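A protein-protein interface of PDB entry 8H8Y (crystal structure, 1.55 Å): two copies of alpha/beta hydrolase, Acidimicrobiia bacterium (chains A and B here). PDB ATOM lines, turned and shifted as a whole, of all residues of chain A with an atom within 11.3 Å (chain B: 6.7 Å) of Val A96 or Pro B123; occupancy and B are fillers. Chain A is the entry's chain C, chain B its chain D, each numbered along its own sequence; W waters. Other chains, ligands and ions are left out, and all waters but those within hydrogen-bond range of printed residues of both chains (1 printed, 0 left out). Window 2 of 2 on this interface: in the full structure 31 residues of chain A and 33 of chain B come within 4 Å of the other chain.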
ATOM      1  N   VAL A  91      20.190  -1.933   7.582  1.00  0.00           N
ATOM      2  CA  VAL A  91      21.369  -1.029   7.679  1.00  0.00           C
ATOM      3  C   VAL A  91      22.421  -1.820   8.439  1.00  0.00           C
ATOM      4  O   VAL A  91      22.086  -2.378   9.487  1.00  0.00           O
ATOM      5  CB  VAL A  91      21.041   0.309   8.350  1.00  0.00           C
ATOM      6  CG1 VAL A  91      22.292   1.093   8.697  1.00  0.00           C
ATOM      7  CG2 VAL A  91      20.126   1.150   7.480  1.00  0.00           C
ATOM      8  N   THR A  92      23.619  -1.951   7.884  1.00  0.00           N
ATOM      9  CA  THR A  92      24.678  -2.798   8.475  1.00  0.00           C
ATOM     10  C   THR A  92      25.903  -1.946   8.788  1.00  0.00           C
ATOM     11  O   THR A  92      26.083  -0.884   8.158  1.00  0.00           O
ATOM     12  CB  THR A  92      25.053  -3.951   7.539  1.00  0.00           C
ATOM     13  OG1 THR A  92      25.480  -3.317   6.346  1.00  0.00           O
ATOM     14  CG2 THR A  92      23.905  -4.880   7.225  1.00  0.00           C
ATOM     15  N   GLY A  93      26.743  -2.457   9.670  1.00  0.00           N
ATOM     16  CA  GLY A  93      28.010  -1.822  10.032  1.00  0.00           C
ATOM     17  C   GLY A  93      28.220  -1.822  11.522  1.00  0.00           C
ATOM     18  O   GLY A  93      27.225  -1.872  12.282  1.00  0.00           O
ATOM     19  N   ARG A  94      29.486  -1.776  11.916  1.00  0.00           N
ATOM     20  CA  ARG A  94      29.876  -1.775  13.344  1.00  0.00           C
ATOM     21  C   ARG A  94      29.270  -0.541  14.012  1.00  0.00           C
ATOM     22  O   ARG A  94      29.192   0.522  13.388  1.00  0.00           O
ATOM     23  CB  ARG A  94      31.401  -1.782  13.454  1.00  0.00           C
ATOM     24  CG  ARG A  94      32.025  -3.066  12.920  1.00  0.00           C
ATOM     25  CD  ARG A  94      33.529  -2.925  12.768  1.00  0.00           C
ATOM     26  NE  ARG A  94      34.122  -2.585  14.053  1.00  0.00           N
ATOM     27  CZ  ARG A  94      35.376  -2.180  14.246  1.00  0.00           C
ATOM     28  NH1 ARG A  94      36.215  -2.061  13.227  1.00  0.00           N
ATOM     29  NH2 ARG A  94      35.788  -1.914  15.473  1.00  0.00           N
ATOM     30  N   PHE A  95      28.781  -0.695  15.244  1.00  0.00           N
ATOM     31  CA  PHE A  95      28.285   0.434  16.060  1.00  0.00           C
ATOM     32  C   PHE A  95      29.302   1.581  16.079  1.00  0.00           C
ATOM     33  O   PHE A  95      28.908   2.726  15.935  1.00  0.00           O
ATOM     34  CB  PHE A  95      28.008  -0.060  17.480  1.00  0.00           C
ATOM     35  CG  PHE A  95      27.606   1.050  18.402  1.00  0.00           C
ATOM     36  CD1 PHE A  95      26.336   1.602  18.334  1.00  0.00           C
ATOM     37  CD2 PHE A  95      28.508   1.579  19.303  1.00  0.00           C
ATOM     38  CE1 PHE A  95      25.986   2.660  19.145  1.00  0.00           C
ATOM     39  CE2 PHE A  95      28.143   2.615  20.140  1.00  0.00           C
ATOM     40  CZ  PHE A  95      26.887   3.155  20.060  1.00  0.00           C
ATOM     41  N   VAL A  96      30.580   1.262  16.330  1.00  0.00           N
ATOM     42  CA  VAL A  96      31.647   2.293  16.506  1.00  0.00           C
ATOM     43  C   VAL A  96      31.902   3.011  15.180  1.00  0.00           C
ATOM     44  O   VAL A  96      32.496   4.089  15.220  1.00  0.00           O
ATOM     45  CB  VAL A  96      32.959   1.717  17.082  1.00  0.00           C
ATOM     46  CG1 VAL A  96      32.821   1.529  18.581  1.00  0.00           C
ATOM     47  CG2 VAL A  96      33.398   0.427  16.391  1.00  0.00           C
ATOM     48  N   ASN A  97      31.403   2.486  14.064  1.00  0.00           N
ATOM     49  CA  ASN A  97      31.568   3.191  12.767  1.00  0.00           C
ATOM     50  C   ASN A  97      30.240   3.825  12.340  1.00  0.00           C
ATOM     51  O   ASN A  97      30.198   4.408  11.248  1.00  0.00           O
ATOM     52  CB  ASN A  97      32.107   2.234  11.705  1.00  0.00           C
ATOM     53  CG  ASN A  97      33.403   1.572  12.120  1.00  0.00           C
ATOM     54  OD1 ASN A  97      34.198   2.158  12.851  1.00  0.00           O
ATOM     55  ND2 ASN A  97      33.622   0.351  11.661  1.00  0.00           N
ATOM     56  N   SER A  98      29.206   3.730  13.176  1.00  0.00           N
ATOM     57  CA  SER A  98      27.859   4.222  12.804  1.00  0.00           C
ATOM     58  C   SER A  98      27.709   5.731  13.055  1.00  0.00           C
ATOM     59  O   SER A  98      28.544   6.309  13.755  1.00  0.00           O
ATOM     60  CB  SER A  98      26.785   3.427  13.553  1.00  0.00           C
ATOM     61  OG  SER A  98      26.762   3.777  14.913  1.00  0.00           O
ATOM     62  N   THR A  99      26.635   6.336  12.563  1.00  0.00           N
ATOM     63  CA  THR A  99      26.292   7.763  12.819  1.00  0.00           C
ATOM     64  C   THR A  99      24.880   7.892  13.412  1.00  0.00           C
ATOM     65  O   THR A  99      24.025   7.008  13.149  1.00  0.00           O
ATOM     66  CB  THR A  99      26.372   8.541  11.500  1.00  0.00           C
ATOM     67  OG1 THR A  99      25.228   8.219  10.717  1.00  0.00           O
ATOM     68  CG2 THR A  99      27.622   8.207  10.711  1.00  0.00           C
ATOM     69  N   ILE A 100      24.617   8.979  14.133  1.00  0.00           N
ATOM     70  CA  ILE A 100      23.254   9.359  14.609  1.00  0.00           C
ATOM     71  C   ILE A 100      22.288   9.485  13.422  1.00  0.00           C
ATOM     72  O   ILE A 100      21.096   9.159  13.584  1.00  0.00           O
ATOM     73  CB  ILE A 100      23.310  10.637  15.467  1.00  0.00           C
ATOM     74  CG1 ILE A 100      21.963  10.943  16.122  1.00  0.00           C
ATOM     75  CG2 ILE A 100      23.803  11.830  14.675  1.00  0.00           C
ATOM     76  CD1 ILE A 100      21.642  10.022  17.256  1.00  0.00           C
ATOM     77  N   GLN A 102      22.202   7.716  10.679  1.00  0.00           N
ATOM     78  CA  GLN A 102      21.817   6.311  10.355  1.00  0.00           C
ATOM     79  C   GLN A 102      20.772   5.865  11.383  1.00  0.00           C
ATOM     80  O   GLN A 102      19.756   5.265  10.989  1.00  0.00           O
ATOM     81  CB  GLN A 102      23.029   5.397  10.361  1.00  0.00           C
ATOM     82  CG  GLN A 102      23.992   5.671   9.207  1.00  0.00           C
ATOM     83  CD  GLN A 102      25.363   5.096   9.444  1.00  0.00           C
ATOM     84  OE1 GLN A 102      25.689   4.595  10.511  1.00  0.00           O
ATOM     85  NE2 GLN A 102      26.202   5.180   8.422  1.00  0.00           N
ATOM     86  N   LEU A 103      20.995   6.161  12.662  1.00  0.00           N
ATOM     87  CA  LEU A 103      20.016   5.745  13.688  1.00  0.00           C
ATOM     88  C   LEU A 103      18.665   6.384  13.388  1.00  0.00           C
ATOM     89  O   LEU A 103      17.652   5.678  13.454  1.00  0.00           O
ATOM     90  CB  LEU A 103      20.530   6.125  15.077  1.00  0.00           C
ATOM     91  CG  LEU A 103      19.531   5.843  16.190  1.00  0.00           C
ATOM     92  CD1 LEU A 103      19.316   4.341  16.373  1.00  0.00           C
ATOM     93  CD2 LEU A 103      19.982   6.500  17.477  1.00  0.00           C
ATOM     94  N   THR A 145      21.921  -8.638  16.713  1.00  0.00           N
ATOM     95  CA  THR A 145      22.061  -9.030  15.295  1.00  0.00           C
ATOM     96  C   THR A 145      23.447  -8.625  14.830  1.00  0.00           C
ATOM     97  O   THR A 145      23.698  -7.441  14.612  1.00  0.00           O
ATOM     98  CB  THR A 145      20.955  -8.408  14.443  1.00  0.00           C
ATOM     99  OG1 THR A 145      19.729  -8.874  15.000  1.00  0.00           O
ATOM    100  CG2 THR A 145      21.055  -8.798  12.993  1.00  0.00           C
ATOM    101  N   GLY A 147      26.397  -7.354  13.014  1.00  0.00           N
ATOM    102  CA  GLY A 147      26.535  -6.453  11.852  1.00  0.00           C
ATOM    103  C   GLY A 147      25.376  -5.481  11.650  1.00  0.00           C
ATOM    104  O   GLY A 147      25.466  -4.655  10.721  1.00  0.00           O
ATOM    105  N   ALA A 148      24.275  -5.556  12.422  1.00  0.00           N
ATOM    106  CA  ALA A 148      23.137  -4.629  12.223  1.00  0.00           C
ATOM    107  C   ALA A 148      22.599  -4.145  13.575  1.00  0.00           C
ATOM    108  O   ALA A 148      21.397  -4.275  13.876  1.00  0.00           O
ATOM    109  CB  ALA A 148      22.089  -5.318  11.387  1.00  0.00           C
ATOM    110  N   PRO A 149      23.456  -3.534  14.424  1.00  0.00           N
ATOM    111  CA  PRO A 149      23.047  -3.206  15.782  1.00  0.00           C
ATOM    112  C   PRO A 149      21.934  -2.145  15.819  1.00  0.00           C
ATOM    113  O   PRO A 149      21.024  -2.219  16.674  1.00  0.00           O
ATOM    114  CB  PRO A 149      24.323  -2.668  16.463  1.00  0.00           C
ATOM    115  CG  PRO A 149      25.175  -2.204  15.285  1.00  0.00           C
ATOM    116  CD  PRO A 149      24.873  -3.186  14.171  1.00  0.00           C
ATOM    117  N   LEU A 150      22.028  -1.127  14.962  1.00  0.00           N
ATOM    118  CA  LEU A 150      21.044  -0.020  14.987  1.00  0.00           C
ATOM    119  C   LEU A 150      19.714  -0.556  14.482  1.00  0.00           C
ATOM    120  O   LEU A 150      18.658  -0.251  15.064  1.00  0.00           O
ATOM    121  CB  LEU A 150      21.542   1.139  14.121  1.00  0.00           C
ATOM    122  CG  LEU A 150      22.499   2.128  14.780  1.00  0.00           C
ATOM    123  CD1 LEU A 150      23.693   1.454  15.375  1.00  0.00           C
ATOM    124  CD2 LEU A 150      22.918   3.196  13.793  1.00  0.00           C
ATOM    125  N   GLN B  67      30.974  13.292  23.678  1.00  0.00           N
ATOM    126  CA  GLN B  67      32.435  13.332  23.408  1.00  0.00           C
ATOM    127  C   GLN B  67      33.124  14.263  24.413  1.00  0.00           C
ATOM    128  O   GLN B  67      34.235  13.921  24.859  1.00  0.00           O
ATOM    129  CB  GLN B  67      32.715  13.730  21.969  1.00  0.00           C
ATOM    130  CG  GLN B  67      34.134  13.378  21.567  1.00  0.00           C
ATOM    131  CD  GLN B  67      34.408  11.895  21.673  1.00  0.00           C
ATOM    132  OE1 GLN B  67      33.770  11.066  21.013  1.00  0.00           O
ATOM    133  NE2 GLN B  67      35.381  11.554  22.498  1.00  0.00           N
ATOM    134  N   PHE B 117      26.006   8.597  24.054  1.00  0.00           N
ATOM    135  CA  PHE B 117      26.902   8.231  25.185  1.00  0.00           C
ATOM    136  C   PHE B 117      27.800   7.049  24.797  1.00  0.00           C
ATOM    137  O   PHE B 117      29.017   7.128  24.890  1.00  0.00           O
ATOM    138  CB  PHE B 117      26.081   7.931  26.437  1.00  0.00           C
ATOM    139  CG  PHE B 117      26.879   7.902  27.716  1.00  0.00           C
ATOM    140  CD1 PHE B 117      27.334   9.074  28.303  1.00  0.00           C
ATOM    141  CD2 PHE B 117      27.153   6.699  28.367  1.00  0.00           C
ATOM    142  CE1 PHE B 117      28.070   9.042  29.473  1.00  0.00           C
ATOM    143  CE2 PHE B 117      27.855   6.675  29.561  1.00  0.00           C
ATOM    144  CZ  PHE B 117      28.295   7.846  30.125  1.00  0.00           C
ATOM    145  N   MET B 118      27.208   5.970  24.280  1.00  0.00           N
ATOM    146  CA  MET B 118      27.987   4.761  23.941  1.00  0.00           C
ATOM    147  C   MET B 118      28.908   5.032  22.733  1.00  0.00           C
ATOM    148  O   MET B 118      30.018   4.477  22.714  1.00  0.00           O
ATOM    149  CB  MET B 118      27.051   3.588  23.669  1.00  0.00           C
ATOM    150  CG  MET B 118      26.407   3.067  24.944  1.00  0.00           C
ATOM    151  SD  MET B 118      25.444   1.533  24.602  1.00  0.00           S
ATOM    152  CE  MET B 118      23.977   2.182  23.809  1.00  0.00           C
ATOM    153  N   ARG B 119      28.469   5.870  21.804  1.00  0.00           N
ATOM    154  CA  ARG B 119      29.247   6.179  20.588  1.00  0.00           C
ATOM    155  C   ARG B 119      30.528   6.888  21.035  1.00  0.00           C
ATOM    156  O   ARG B 119      31.567   6.610  20.459  1.00  0.00           O
ATOM    157  CB  ARG B 119      28.381   6.959  19.595  1.00  0.00           C
ATOM    158  CG  ARG B 119      28.898   7.014  18.163  1.00  0.00           C
ATOM    159  CD  ARG B 119      29.448   5.709  17.634  1.00  0.00           C
ATOM    160  NE  ARG B 119      30.126   5.966  16.380  1.00  0.00           N
ATOM    161  CZ  ARG B 119      31.363   6.419  16.285  1.00  0.00           C
ATOM    162  NH1 ARG B 119      32.075   6.634  17.382  1.00  0.00           N
ATOM    163  NH2 ARG B 119      31.884   6.641  15.095  1.00  0.00           N
ATOM    164  N   ALA B 120      30.483   7.687  22.095  1.00  0.00           N
ATOM    165  CA  ALA B 120      31.671   8.418  22.596  1.00  0.00           C
ATOM    166  C   ALA B 120      32.482   7.526  23.538  1.00  0.00           C
ATOM    167  O   ALA B 120      33.719   7.414  23.348  1.00  0.00           O
ATOM    168  CB  ALA B 120      31.248   9.694  23.251  1.00  0.00           C
ATOM    169  N   VAL B 121      31.833   6.861  24.488  1.00  0.00           N
ATOM    170  CA  VAL B 121      32.561   6.154  25.575  1.00  0.00           C
ATOM    171  C   VAL B 121      33.120   4.814  25.059  1.00  0.00           C
ATOM    172  O   VAL B 121      34.233   4.444  25.431  1.00  0.00           O
ATOM    173  CB  VAL B 121      31.668   5.987  26.817  1.00  0.00           C
ATOM    174  CG1 VAL B 121      32.309   5.103  27.874  1.00  0.00           C
ATOM    175  CG2 VAL B 121      31.321   7.346  27.406  1.00  0.00           C
ATOM    176  N   VAL B 122      32.372   4.068  24.244  1.00  0.00           N
ATOM    177  CA  VAL B 122      32.805   2.685  23.883  1.00  0.00           C
ATOM    178  C   VAL B 122      34.209   2.709  23.260  1.00  0.00           C
ATOM    179  O   VAL B 122      35.057   1.948  23.711  1.00  0.00           O
ATOM    180  CB  VAL B 122      31.777   1.960  22.994  1.00  0.00           C
ATOM    181  CG1 VAL B 122      32.370   0.702  22.379  1.00  0.00           C
ATOM    182  CG2 VAL B 122      30.504   1.612  23.777  1.00  0.00           C
ATOM    183  N   PRO B 123      34.502   3.561  22.236  1.00  0.00           N
ATOM    184  CA  PRO B 123      35.831   3.610  21.600  1.00  0.00           C
ATOM    185  C   PRO B 123      36.967   3.878  22.585  1.00  0.00           C
ATOM    186  O   PRO B 123      38.031   3.320  22.454  1.00  0.00           O
ATOM    187  CB  PRO B 123      35.735   4.798  20.633  1.00  0.00           C
ATOM    188  CG  PRO B 123      34.267   4.837  20.288  1.00  0.00           C
ATOM    189  CD  PRO B 123      33.582   4.521  21.604  1.00  0.00           C
ATOM    190  N   VAL B 124      36.707   4.723  23.574  1.00  0.00           N
ATOM    191  CA  VAL B 124      37.699   5.037  24.636  1.00  0.00           C
ATOM    192  C   VAL B 124      38.034   3.746  25.393  1.00  0.00           C
ATOM    193  O   VAL B 124      39.204   3.426  25.558  1.00  0.00           O
ATOM    194  CB  VAL B 124      37.191   6.127  25.590  1.00  0.00           C
ATOM    195  CG1 VAL B 124      38.169   6.382  26.713  1.00  0.00           C
ATOM    196  CG2 VAL B 124      36.881   7.428  24.874  1.00  0.00           C
ATOM    197  N   MET B 125      37.024   2.974  25.790  1.00  0.00           N
ATOM    198  CA  MET B 125      37.234   1.770  26.624  1.00  0.00           C
ATOM    199  C   MET B 125      37.797   0.614  25.787  1.00  0.00           C
ATOM    200  O   MET B 125      38.687  -0.088  26.296  1.00  0.00           O
ATOM    201  CB  MET B 125      35.916   1.362  27.285  1.00  0.00           C
ATOM    202  CG  MET B 125      35.394   2.436  28.243  1.00  0.00           C
ATOM    203  SD  MET B 125      34.016   1.837  29.267  1.00  0.00           S
ATOM    204  CE  MET B 125      34.061   3.010  30.611  1.00  0.00           C
ATOM    205  N   THR B 126      37.331   0.412  24.563  1.00  0.00           N
ATOM    206  CA  THR B 126      37.799  -0.718  23.719  1.00  0.00           C
ATOM    207  C   THR B 126      39.303  -0.536  23.454  1.00  0.00           C
ATOM    208  O   THR B 126      40.020  -1.556  23.415  1.00  0.00           O
ATOM    209  CB  THR B 126      36.974  -0.848  22.437  1.00  0.00           C
ATOM    210  OG1 THR B 126      37.015   0.421  21.782  1.00  0.00           O
ATOM    211  CG2 THR B 126      35.540  -1.265  22.698  1.00  0.00           C
ATOM    212  N   GLU B 127      39.767   0.712  23.307  1.00  0.00           N
ATOM    213  CA  GLU B 127      41.214   1.030  23.172  1.00  0.00           C
ATOM    214  C   GLU B 127      41.996   0.467  24.353  1.00  0.00           C
ATOM    215  O   GLU B 127      43.069  -0.065  24.118  1.00  0.00           O
ATOM    216  CB  GLU B 127      41.473   2.532  23.105  1.00  0.00           C
ATOM    217  CG  GLU B 127      41.147   3.136  21.753  1.00  0.00           C
ATOM    218  CD  GLU B 127      41.402   4.635  21.684  1.00  0.00           C
ATOM    219  OE1 GLU B 127      42.595   5.028  21.728  1.00  0.00           O
ATOM    220  OE2 GLU B 127      40.411   5.408  21.608  1.00  0.00           O
ATOM    221  N   ARG B 128      41.492   0.596  25.575  1.00  0.00           N
ATOM    222  CA  ARG B 128      42.202   0.150  26.801  1.00  0.00           C
ATOM    223  C   ARG B 128      41.848  -1.300  27.132  1.00  0.00           C
ATOM    224  O   ARG B 128      42.261  -1.767  28.185  1.00  0.00           O
ATOM    225  CB  ARG B 128      41.841   1.071  27.966  1.00  0.00           C
ATOM    226  CG  ARG B 128      42.368   2.485  27.786  1.00  0.00           C
ATOM    227  CD  ARG B 128      41.293   3.545  27.903  1.00  0.00           C
ATOM    228  NE  ARG B 128      41.560   4.631  26.970  1.00  0.00           N
ATOM    229  CZ  ARG B 128      42.391   5.648  27.194  1.00  0.00           C
ATOM    230  NH1 ARG B 128      43.031   5.751  28.351  1.00  0.00           N
ATOM    231  NH2 ARG B 128      42.568   6.569  26.257  1.00  0.00           N
ATOM    232  N   GLU B 168      28.890  -6.797  20.330  1.00  0.00           N
ATOM    233  CA  GLU B 168      29.935  -6.318  19.389  1.00  0.00           C
ATOM    234  C   GLU B 168      31.285  -6.228  20.110  1.00  0.00           C
ATOM    235  O   GLU B 168      32.293  -6.593  19.476  1.00  0.00           O
ATOM    236  CB  GLU B 168      29.520  -4.989  18.750  1.00  0.00           C
ATOM    237  CG  GLU B 168      30.588  -4.402  17.832  1.00  0.00           C
ATOM    238  CD  GLU B 168      30.154  -3.150  17.086  1.00  0.00           C
ATOM    239  OE1 GLU B 168      29.037  -3.187  16.551  1.00  0.00           O
ATOM    240  OE2 GLU B 168      30.923  -2.112  17.103  1.00  0.00           O
ATOM    241  N   VAL B 169      31.340  -5.730  21.351  1.00  0.00           N
ATOM    242  CA  VAL B 169      32.614  -5.318  22.003  1.00  0.00           C
ATOM    243  C   VAL B 169      33.000  -6.308  23.102  1.00  0.00           C
ATOM    244  O   VAL B 169      33.990  -6.059  23.798  1.00  0.00           O
ATOM    245  CB  VAL B 169      32.566  -3.879  22.549  1.00  0.00           C
ATOM    246  CG1 VAL B 169      32.098  -2.934  21.453  1.00  0.00           C
ATOM    247  CG2 VAL B 169      31.691  -3.762  23.791  1.00  0.00           C
HETATM  248  O   HOH W   1      31.584   6.706  12.312  1.00  0.00           O
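Water W1 lies within hydrogen-bond range of NH2 of Arg B119, O of Asn A97 and O of Ser A98.
Among the printed residues, pairs that only touch across the chains: Arg A94 with Glu B168 (3.6 Å), Phe A95 with Met B118 (3.6 Å), Val A96 with Val B122 (3.9 Å) and Val A96 with Pro B123 (3.99 Å).
Printed residues of chain B that touch a printed residue of chain A: Met B118, Arg B119, Val B122, Pro B123 and Glu B168. Hydrophobic or aromatic side chains of chain B within 4 Å of the printed part of chain A: Met B118, Val B122 and Pro B123. Among the printed residues, 9 pairs touch across the chains. Among the printed residues, no Asp or Glu carboxylate lies within 4 Å of a Lys or Arg side-chain nitrogen of the other chain.
The side-chain hydroxyl (OG1) of Thr B126 sits at hydrogen-bond distance from the backbone carbonyl oxygen (O) of Pro B123. The backbone carbonyl oxygen of Phe A95 sits at hydrogen-bond distance from the side-chain hydroxyl of Ser A98 (2.6 Å). The side-chain hydroxyl of Thr B126 is in hydrogen-bond range of the backbone carbonyl oxygen of Val B122, 3.1 Å away.
The guanidinium group of Arg B119 lies close to the backbone carbonyl oxygen of Phe A95. The backbone carbonyl oxygen (O) of Ser A98 sits at hydrogen-bond distance from the guanidinium group (NE) of Arg B119, at 3.1 Å. The backbone carbonyl oxygen (O) of Val A96 lies within hydrogen-bond range of the guanidinium group (NH2) of Arg B119 (2.6 Å). The side-chain carboxylate (OE1) of Glu B168 is in hydrogen-bond range of the backbone NH (N) of Phe A95, 2.8 Å away. The side-chain carboxylate of Glu B168 is in hydrogen-bond range of the backbone NH of Val A96 (3.5 Å).
Of the printed residues of chain B, Arg A94 touches Glu B168 (3.6 Å). Of the printed residues of chain B, Val A96 touches Arg B119 (2.6 Å), Val B122 (3.9 Å), Pro B123 (3.99 Å) and Glu B168 (3.5 Å). Printed residues of chain A within 4 Å of Met B118: Phe A95. Val B121 touches none of the printed residues of chain A. Of the printed residues of chain A, Pro B123 touches Val A96 (3.99 Å). Thr B126 touches none of the printed residues of chain A. Printed residues of chain A within 4 Å of Glu B168: Arg A94, Phe A95 and Val A96. The nearest printed residue of chain B that does not touch Val A96 is Val B169 (5.4 Å). The nearest printed residue of chain A that does not touch Pro B123 is Phe A95 (5.9 Å).
No position is printed for both chains. Of the 9 pairs that touch across the chains among the printed residues, none has its exchanged pair printed and touching as well.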
